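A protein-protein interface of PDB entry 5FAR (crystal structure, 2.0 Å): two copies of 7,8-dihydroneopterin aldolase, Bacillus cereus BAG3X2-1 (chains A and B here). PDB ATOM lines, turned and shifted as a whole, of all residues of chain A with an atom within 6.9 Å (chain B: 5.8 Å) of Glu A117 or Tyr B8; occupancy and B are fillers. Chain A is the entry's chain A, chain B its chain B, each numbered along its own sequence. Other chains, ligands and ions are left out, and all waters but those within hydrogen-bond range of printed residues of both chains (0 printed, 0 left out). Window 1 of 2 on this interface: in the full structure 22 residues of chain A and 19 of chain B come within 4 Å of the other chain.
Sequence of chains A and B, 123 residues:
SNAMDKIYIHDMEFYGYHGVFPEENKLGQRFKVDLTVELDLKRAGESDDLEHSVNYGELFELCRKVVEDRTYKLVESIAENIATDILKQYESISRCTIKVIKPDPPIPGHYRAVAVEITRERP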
ATOM      1  N   ASP A  34      -3.449  13.049  26.046  1.00  0.00           N
ATOM      2  CA  ASP A  34      -2.214  12.558  26.686  1.00  0.00           C
ATOM      3  C   ASP A  34      -1.618  13.662  27.573  1.00  0.00           C
ATOM      4  O   ASP A  34      -1.197  14.700  27.056  1.00  0.00           O
ATOM      5  CB  ASP A  34      -1.176  12.125  25.641  1.00  0.00           C
ATOM      6  CG  ASP A  34      -1.625  10.915  24.810  1.00  0.00           C
ATOM      7  OD1 ASP A  34      -2.466  10.135  25.294  1.00  0.00           O
ATOM      8  OD2 ASP A  34      -1.114  10.736  23.680  1.00  0.00           O
ATOM      9  N   THR A  36       1.286  14.868  30.457  1.00  0.00           N
ATOM     10  CA  THR A  36       2.716  14.624  30.675  1.00  0.00           C
ATOM     11  C   THR A  36       3.311  15.762  31.521  1.00  0.00           C
ATOM     12  O   THR A  36       3.830  16.745  30.977  1.00  0.00           O
ATOM     13  CB  THR A  36       3.475  14.528  29.328  1.00  0.00           C
ATOM     14  OG1 THR A  36       2.836  13.585  28.471  1.00  0.00           O
ATOM     15  CG2 THR A  36       4.917  14.110  29.525  1.00  0.00           C
ATOM     16  N   ALA A  79      -6.350  22.264  25.239  1.00  0.00           N
ATOM     17  CA  ALA A  79      -4.955  22.085  25.624  1.00  0.00           C
ATOM     18  C   ALA A  79      -4.444  23.200  26.524  1.00  0.00           C
ATOM     19  O   ALA A  79      -3.760  22.923  27.508  1.00  0.00           O
ATOM     20  CB  ALA A  79      -4.081  21.976  24.384  1.00  0.00           C
ATOM     21  N   THR A  97       3.155  18.985  29.519  1.00  0.00           N
ATOM     22  CA  THR A  97       2.922  18.780  28.091  1.00  0.00           C
ATOM     23  C   THR A  97       1.569  18.103  27.929  1.00  0.00           C
ATOM     24  O   THR A  97       1.334  17.029  28.491  1.00  0.00           O
ATOM     25  CB  THR A  97       4.038  17.938  27.437  1.00  0.00           C
ATOM     26  OG1 THR A  97       5.243  18.707  27.396  1.00  0.00           O
ATOM     27  CG2 THR A  97       3.681  17.532  26.015  1.00  0.00           C
ATOM     28  N   ILE A  98       0.680  18.758  27.183  1.00  0.00           N
ATOM     29  CA  ILE A  98      -0.660  18.252  26.918  1.00  0.00           C
ATOM     30  C   ILE A  98      -0.716  17.964  25.434  1.00  0.00           C
ATOM     31  O   ILE A  98      -0.280  18.788  24.632  1.00  0.00           O
ATOM     32  CB  ILE A  98      -1.767  19.288  27.243  1.00  0.00           C
ATOM     33  CG1 ILE A  98      -1.405  20.161  28.450  1.00  0.00           C
ATOM     34  CG2 ILE A  98      -3.112  18.589  27.447  1.00  0.00           C
ATOM     35  CD1 ILE A  98      -1.129  19.411  29.737  1.00  0.00           C
ATOM     36  N   LYS A  99      -1.228  16.790  25.070  1.00  0.00           N
ATOM     37  CA  LYS A  99      -1.541  16.491  23.682  1.00  0.00           C
ATOM     38  C   LYS A  99      -3.014  16.154  23.595  1.00  0.00           C
ATOM     39  O   LYS A  99      -3.434  15.122  24.108  1.00  0.00           O
ATOM     40  CB  LYS A  99      -0.699  15.319  23.168  1.00  0.00           C
ATOM     41  CG  LYS A  99      -0.972  14.894  21.723  1.00  0.00           C
ATOM     42  CD  LYS A  99      -0.498  13.465  21.514  1.00  0.00           C
ATOM     43  CE  LYS A  99      -0.538  13.023  20.057  1.00  0.00           C
ATOM     44  NZ  LYS A  99       0.620  12.136  19.732  1.00  0.00           N
ATOM     45  N   VAL A 100      -3.790  17.018  22.935  1.00  0.00           N
ATOM     46  CA  VAL A 100      -5.220  16.773  22.709  1.00  0.00           C
ATOM     47  C   VAL A 100      -5.415  16.186  21.301  1.00  0.00           C
ATOM     48  O   VAL A 100      -4.821  16.653  20.327  1.00  0.00           O
ATOM     49  CB  VAL A 100      -6.067  18.053  22.918  1.00  0.00           C
ATOM     50  CG1 VAL A 100      -7.521  17.817  22.535  1.00  0.00           C
ATOM     51  CG2 VAL A 100      -5.994  18.496  24.362  1.00  0.00           C
ATOM     52  N   ALA A 113      -5.829  10.039  13.253  1.00  0.00           N
ATOM     53  CA  ALA A 113      -6.229  11.135  14.112  1.00  0.00           C
ATOM     54  C   ALA A 113      -5.506  12.432  13.726  1.00  0.00           C
ATOM     55  O   ALA A 113      -4.429  12.394  13.119  1.00  0.00           O
ATOM     56  CB  ALA A 113      -5.933  10.790  15.566  1.00  0.00           C
ATOM     57  N   VAL A 114      -6.119  13.567  14.061  1.00  0.00           N
ATOM     58  CA  VAL A 114      -5.419  14.862  14.078  1.00  0.00           C
ATOM     59  C   VAL A 114      -5.226  15.222  15.538  1.00  0.00           C
ATOM     60  O   VAL A 114      -5.885  14.631  16.415  1.00  0.00           O
ATOM     61  CB  VAL A 114      -6.163  15.967  13.287  1.00  0.00           C
ATOM     62  CG1 VAL A 114      -6.581  15.438  11.927  1.00  0.00           C
ATOM     63  CG2 VAL A 114      -7.374  16.510  14.035  1.00  0.00           C
ATOM     64  N   ALA A 115      -4.322  16.171  15.814  1.00  0.00           N
ATOM     65  CA  ALA A 115      -3.883  16.412  17.174  1.00  0.00           C
ATOM     66  C   ALA A 115      -3.130  17.755  17.410  1.00  0.00           C
ATOM     67  O   ALA A 115      -2.445  18.260  16.530  1.00  0.00           O
ATOM     68  CB  ALA A 115      -3.017  15.243  17.630  1.00  0.00           C
ATOM     69  N   VAL A 116      -3.286  18.300  18.612  1.00  0.00           N
ATOM     70  CA  VAL A 116      -2.408  19.370  19.111  1.00  0.00           C
ATOM     71  C   VAL A 116      -1.600  18.865  20.289  1.00  0.00           C
ATOM     72  O   VAL A 116      -2.031  17.957  20.988  1.00  0.00           O
ATOM     73  CB  VAL A 116      -3.154  20.680  19.463  1.00  0.00           C
ATOM     74  CG1 VAL A 116      -3.727  21.305  18.204  1.00  0.00           C
ATOM     75  CG2 VAL A 116      -4.243  20.470  20.518  1.00  0.00           C
ATOM     76  N   GLU A 117      -0.401  19.419  20.448  1.00  0.00           N
ATOM     77  CA  GLU A 117       0.472  19.157  21.581  1.00  0.00           C
ATOM     78  C   GLU A 117       1.219  20.444  21.958  1.00  0.00           C
ATOM     79  O   GLU A 117       1.995  20.968  21.153  1.00  0.00           O
ATOM     80  CB  GLU A 117       1.473  18.054  21.242  1.00  0.00           C
ATOM     81  CG  GLU A 117       2.356  17.615  22.408  1.00  0.00           C
ATOM     82  CD  GLU A 117       3.333  16.525  22.025  1.00  0.00           C
ATOM     83  OE1 GLU A 117       4.038  16.690  21.004  1.00  0.00           O
ATOM     84  OE2 GLU A 117       3.403  15.501  22.736  1.00  0.00           O
ATOM     85  N   ILE A 118       0.955  20.940  23.171  1.00  0.00           N
ATOM     86  CA  ILE A 118       1.646  22.103  23.741  1.00  0.00           C
ATOM     87  C   ILE A 118       2.491  21.682  24.938  1.00  0.00           C
ATOM     88  O   ILE A 118       2.197  20.675  25.586  1.00  0.00           O
ATOM     89  CB  ILE A 118       0.662  23.224  24.177  1.00  0.00           C
ATOM     90  CG1 ILE A 118      -0.170  22.818  25.408  1.00  0.00           C
ATOM     91  CG2 ILE A 118      -0.241  23.615  23.008  1.00  0.00           C
ATOM     92  CD1 ILE A 118      -1.116  23.896  25.882  1.00  0.00           C
ATOM     93  N   THR A 119       3.533  22.471  25.214  1.00  0.00           N
ATOM     94  CA  THR A 119       4.359  22.336  26.410  1.00  0.00           C
ATOM     95  C   THR A 119       4.379  23.705  27.110  1.00  0.00           C
ATOM     96  O   THR A 119       4.691  24.717  26.478  1.00  0.00           O
ATOM     97  CB  THR A 119       5.786  21.863  26.044  1.00  0.00           C
ATOM     98  OG1 THR A 119       5.724  20.545  25.480  1.00  0.00           O
ATOM     99  CG2 THR A 119       6.704  21.824  27.263  1.00  0.00           C
ATOM    100  N   ARG A 120       4.022  23.726  28.396  1.00  0.00           N
ATOM    101  CA  ARG A 120       3.945  24.956  29.201  1.00  0.00           C
ATOM    102  C   ARG A 120       4.766  24.839  30.485  1.00  0.00           C
ATOM    103  O   ARG A 120       4.978  23.740  31.000  1.00  0.00           O
ATOM    104  CB  ARG A 120       2.488  25.277  29.561  1.00  0.00           C
ATOM    105  CG  ARG A 120       1.579  25.576  28.371  1.00  0.00           C
ATOM    106  CD  ARG A 120       1.868  26.927  27.730  1.00  0.00           C
ATOM    107  NE  ARG A 120       1.119  27.137  26.479  1.00  0.00           N
ATOM    108  CZ  ARG A 120       1.542  26.833  25.244  1.00  0.00           C
ATOM    109  NH1 ARG A 120       2.736  26.281  25.024  1.00  0.00           N
ATOM    110  NH2 ARG A 120       0.751  27.093  24.200  1.00  0.00           N
ATOM    111  N   MET B   4       8.636  23.599  20.350  1.00  0.00           N
ATOM    112  CA  MET B   4       7.454  24.491  20.119  1.00  0.00           C
ATOM    113  C   MET B   4       6.177  23.760  20.458  1.00  0.00           C
ATOM    114  O   MET B   4       6.215  22.645  20.991  1.00  0.00           O
ATOM    115  CB  MET B   4       7.445  24.963  18.656  1.00  0.00           C
ATOM    116  CG  MET B   4       7.161  26.458  18.525  1.00  0.00           C
ATOM    117  SD  MET B   4       7.344  26.986  16.637  1.00  0.00           S
ATOM    118  CE  MET B   4       9.174  27.706  16.762  1.00  0.00           C
ATOM    119  N   ASP B   5       5.044  24.415  20.198  1.00  0.00           N
ATOM    120  CA  ASP B   5       3.739  23.763  20.164  1.00  0.00           C
ATOM    121  C   ASP B   5       3.599  23.057  18.822  1.00  0.00           C
ATOM    122  O   ASP B   5       4.239  23.459  17.847  1.00  0.00           O
ATOM    123  CB  ASP B   5       2.614  24.789  20.311  1.00  0.00           C
ATOM    124  CG  ASP B   5       2.689  25.561  21.605  1.00  0.00           C
ATOM    125  OD1 ASP B   5       3.447  25.148  22.515  1.00  0.00           O
ATOM    126  OD2 ASP B   5       1.977  26.586  21.717  1.00  0.00           O
ATOM    127  N   LYS B   6       2.749  22.026  18.769  1.00  0.00           N
ATOM    128  CA  LYS B   6       2.675  21.136  17.606  1.00  0.00           C
ATOM    129  C   LYS B   6       1.240  20.803  17.193  1.00  0.00           C
ATOM    130  O   LYS B   6       0.414  20.480  18.044  1.00  0.00           O
ATOM    131  CB  LYS B   6       3.429  19.839  17.906  1.00  0.00           C
ATOM    132  CG  LYS B   6       4.945  20.000  17.960  1.00  0.00           C
ATOM    133  CD  LYS B   6       5.616  18.762  18.535  1.00  0.00           C
ATOM    134  CE  LYS B   6       7.132  18.862  18.500  1.00  0.00           C
ATOM    135  NZ  LYS B   6       7.652  20.075  19.192  1.00  0.00           N
ATOM    136  N   ILE B   7       0.957  20.906  15.892  1.00  0.00           N
ATOM    137  CA  ILE B   7      -0.216  20.258  15.289  1.00  0.00           C
ATOM    138  C   ILE B   7       0.264  18.987  14.591  1.00  0.00           C
ATOM    139  O   ILE B   7       1.352  18.966  14.012  1.00  0.00           O
ATOM    140  CB  ILE B   7      -0.981  21.172  14.297  1.00  0.00           C
ATOM    141  CG1 ILE B   7      -1.729  22.266  15.061  1.00  0.00           C
ATOM    142  CG2 ILE B   7      -2.014  20.377  13.480  1.00  0.00           C
ATOM    143  CD1 ILE B   7      -2.256  23.388  14.191  1.00  0.00           C
ATOM    144  N   TYR B   8      -0.575  17.950  14.648  1.00  0.00           N
ATOM    145  CA  TYR B   8      -0.291  16.614  14.132  1.00  0.00           C
ATOM    146  C   TYR B   8      -1.440  16.102  13.248  1.00  0.00           C
ATOM    147  O   TYR B   8      -2.612  16.398  13.511  1.00  0.00           O
ATOM    148  CB  TYR B   8      -0.194  15.638  15.300  1.00  0.00           C
ATOM    149  CG  TYR B   8       1.056  15.684  16.153  1.00  0.00           C
ATOM    150  CD1 TYR B   8       2.281  15.262  15.650  1.00  0.00           C
ATOM    151  CD2 TYR B   8       0.996  16.078  17.490  1.00  0.00           C
ATOM    152  CE1 TYR B   8       3.420  15.256  16.445  1.00  0.00           C
ATOM    153  CE2 TYR B   8       2.133  16.083  18.286  1.00  0.00           C
ATOM    154  CZ  TYR B   8       3.339  15.674  17.758  1.00  0.00           C
ATOM    155  OH  TYR B   8       4.470  15.684  18.540  1.00  0.00           O
ATOM    156  N   ILE B   9      -1.091  15.347  12.207  1.00  0.00           N
ATOM    157  CA  ILE B   9      -2.016  14.382  11.585  1.00  0.00           C
ATOM    158  C   ILE B   9      -1.304  13.019  11.578  1.00  0.00           C
ATOM    159  O   ILE B   9      -0.188  12.885  11.072  1.00  0.00           O
ATOM    160  CB  ILE B   9      -2.507  14.801  10.174  1.00  0.00           C
ATOM    161  CG1 ILE B   9      -3.178  16.182  10.224  1.00  0.00           C
ATOM    162  CG2 ILE B   9      -3.529  13.794   9.633  1.00  0.00           C
ATOM    163  CD1 ILE B   9      -3.583  16.748   8.881  1.00  0.00           C
ATOM    164  N   HIS B  10      -1.965  12.020  12.157  1.00  0.00           N
ATOM    165  CA  HIS B  10      -1.379  10.709  12.393  1.00  0.00           C
ATOM    166  C   HIS B  10      -1.902   9.692  11.401  1.00  0.00           C
ATOM    167  O   HIS B  10      -3.117   9.512  11.285  1.00  0.00           O
ATOM    168  CB  HIS B  10      -1.754  10.200  13.788  1.00  0.00           C
ATOM    169  CG  HIS B  10      -1.157  10.991  14.906  1.00  0.00           C
ATOM    170  ND1 HIS B  10       0.182  11.326  14.953  1.00  0.00           N
ATOM    171  CD2 HIS B  10      -1.713  11.498  16.029  1.00  0.00           C
ATOM    172  CE1 HIS B  10       0.423  12.003  16.060  1.00  0.00           C
ATOM    173  NE2 HIS B  10      -0.711  12.129  16.725  1.00  0.00           N
ATOM    174  N   LEU B  35       2.213  13.572   9.709  1.00  0.00           N
ATOM    175  CA  LEU B  35       2.517  15.009   9.602  1.00  0.00           C
ATOM    176  C   LEU B  35       2.788  15.586  10.982  1.00  0.00           C
ATOM    177  O   LEU B  35       2.037  15.319  11.932  1.00  0.00           O
ATOM    178  CB  LEU B  35       1.340  15.763   8.968  1.00  0.00           C
ATOM    179  CG  LEU B  35       1.396  17.289   8.693  1.00  0.00           C
ATOM    180  CD1 LEU B  35       0.290  17.687   7.724  1.00  0.00           C
ATOM    181  CD2 LEU B  35       1.268  18.137   9.958  1.00  0.00           C
ATOM    182  N   THR B  36       3.849  16.393  11.077  1.00  0.00           N
ATOM    183  CA  THR B  36       4.149  17.169  12.286  1.00  0.00           C
ATOM    184  C   THR B  36       4.595  18.574  11.856  1.00  0.00           C
ATOM    185  O   THR B  36       5.506  18.713  11.045  1.00  0.00           O
ATOM    186  CB  THR B  36       5.215  16.474  13.162  1.00  0.00           C
ATOM    187  OG1 THR B  36       4.785  15.133  13.466  1.00  0.00           O
ATOM    188  CG2 THR B  36       5.450  17.243  14.474  1.00  0.00           C
ATOM    189  N   VAL B  37       3.897  19.596  12.351  1.00  0.00           N
ATOM    190  CA  VAL B  37       4.198  20.999  12.018  1.00  0.00           C
ATOM    191  C   VAL B  37       4.337  21.804  13.302  1.00  0.00           C
ATOM    192  O   VAL B  37       3.562  21.595  14.247  1.00  0.00           O
ATOM    193  CB  VAL B  37       3.132  21.650  11.098  1.00  0.00           C
ATOM    194  CG1 VAL B  37       3.158  21.020   9.704  1.00  0.00           C
ATOM    195  CG2 VAL B  37       1.733  21.627  11.718  1.00  0.00           C
ATOM    196  N   LEU B  41       0.722  28.197  19.329  1.00  0.00           N
ATOM    197  CA  LEU B  41      -0.710  27.983  19.528  1.00  0.00           C
ATOM    198  C   LEU B  41      -1.233  28.617  20.816  1.00  0.00           C
ATOM    199  O   LEU B  41      -2.401  28.412  21.180  1.00  0.00           O
ATOM    200  CB  LEU B  41      -0.996  26.472  19.528  1.00  0.00           C
ATOM    201  CG  LEU B  41      -0.523  25.712  18.277  1.00  0.00           C
ATOM    202  CD1 LEU B  41      -0.745  24.212  18.430  1.00  0.00           C
ATOM    203  CD2 LEU B  41      -1.213  26.235  17.023  1.00  0.00           C
ATOM    204  N   TYR B  56      -6.527  21.997  10.039  1.00  0.00           N
ATOM    205  CA  TYR B  56      -6.057  20.603   9.894  1.00  0.00           C
ATOM    206  C   TYR B  56      -6.593  19.895   8.626  1.00  0.00           C
ATOM    207  O   TYR B  56      -5.942  18.993   8.099  1.00  0.00           O
ATOM    208  CB  TYR B  56      -6.248  19.758  11.181  1.00  0.00           C
ATOM    209  CG  TYR B  56      -7.656  19.669  11.772  1.00  0.00           C
ATOM    210  CD1 TYR B  56      -8.746  19.251  11.001  1.00  0.00           C
ATOM    211  CD2 TYR B  56      -7.884  19.943  13.120  1.00  0.00           C
ATOM    212  CE1 TYR B  56     -10.018  19.146  11.536  1.00  0.00           C
ATOM    213  CE2 TYR B  56      -9.156  19.838  13.663  1.00  0.00           C
ATOM    214  CZ  TYR B  56     -10.222  19.439  12.859  1.00  0.00           C
ATOM    215  OH  TYR B  56     -11.495  19.337  13.362  1.00  0.00           O
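1 position is printed for both chains.
Among the printed residues, pairs that only touch across the chains: Val A116 with Lys B6, Ala A115 with Ile B7, Val A114 with Tyr B8, Glu A117 with Asp B5, Ala A113 with Ile B9, Val A114 with Tyr B56, Ile A118 with Asp B5, Thr A119 with Asp B5, Val A116 with Ile B7, Val A114 with Ile B9, Ala A115 with Lys B6 and Ala A115 with His B10.
Glu A117 touches just these residues of chain B: Asp B5, Lys B6 and Tyr B8. Tyr B8 touches just these residues of chain A: Val A114, Ala A115 and Glu A117. Printed residues of chain A within 4 Å of Lys B6: Ala A115 (3.9 Å), Val A116 (3.2 Å) and Glu A117 (2.7 Å). Of the printed residues of chain B, Lys A99 touches His B10. Of the printed residues of chain A, Asp B5 touches Glu A117, Ile A118, Thr A119 and Arg A120. Of the printed residues of chain A, Ile B7 touches Ala A115 (3.2 Å) and Val A116 (3.8 Å). Val A100 touches none of the printed residues of chain B. The nearest printed residue of chain B that does not touch Val A114 is His B10 (4.8 Å).
NH2 of Arg A120 is in salt-bridge range of OD2 of Asp B5 (2.8 Å). The backbone NH (N) of Tyr B8 sits at hydrogen-bond distance from the backbone carbonyl oxygen (O) of Ala A115 (2.7 Å). The side-chain carboxylate of Glu A117 is in hydrogen-bond range of the side-chain hydroxyl of Tyr B8. O of Glu A117 sits at hydrogen-bond distance from N of Lys B6, 2.7 Å away. The side-chain amino group (NZ) of Lys A99 lies within hydrogen-bond range of a ring nitrogen (NE2) of His B10 (3.3 Å). O of Ala A113 sits at hydrogen-bond distance from N of His B10 (2.7 Å).
Hydrophobic or aromatic side chains of chain B that line the printed part of chain A: Ile B7, Tyr B8, Ile B9, His B10 and Tyr B56. Among the printed residues, Asp or Glu carboxylates within 4 Å of a Lys or Arg side-chain nitrogen of the other chain: Arg A120 with Asp B5.
OG1 of Thr A119 sits at hydrogen-bond distance from OG1 of Thr A97, at 2.7 Å. The backbone carbonyl oxygen (O) of Val A116 is in hydrogen-bond range of the backbone NH (N) of Val A100, at 2.8 Å. The backbone carbonyl oxygen of Ile B7 lies within hydrogen-bond range of the backbone NH of Val B37 (3.1 Å). The backbone carbonyl oxygen (O) of Ile B9 sits at hydrogen-bond distance from the backbone NH (N) of Leu B35. O of Ile A98 is in hydrogen-bond range of N of Ile A118. OD2 of Asp B5 lies within hydrogen-bond range of N of Leu B41, at 3.1 Å.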
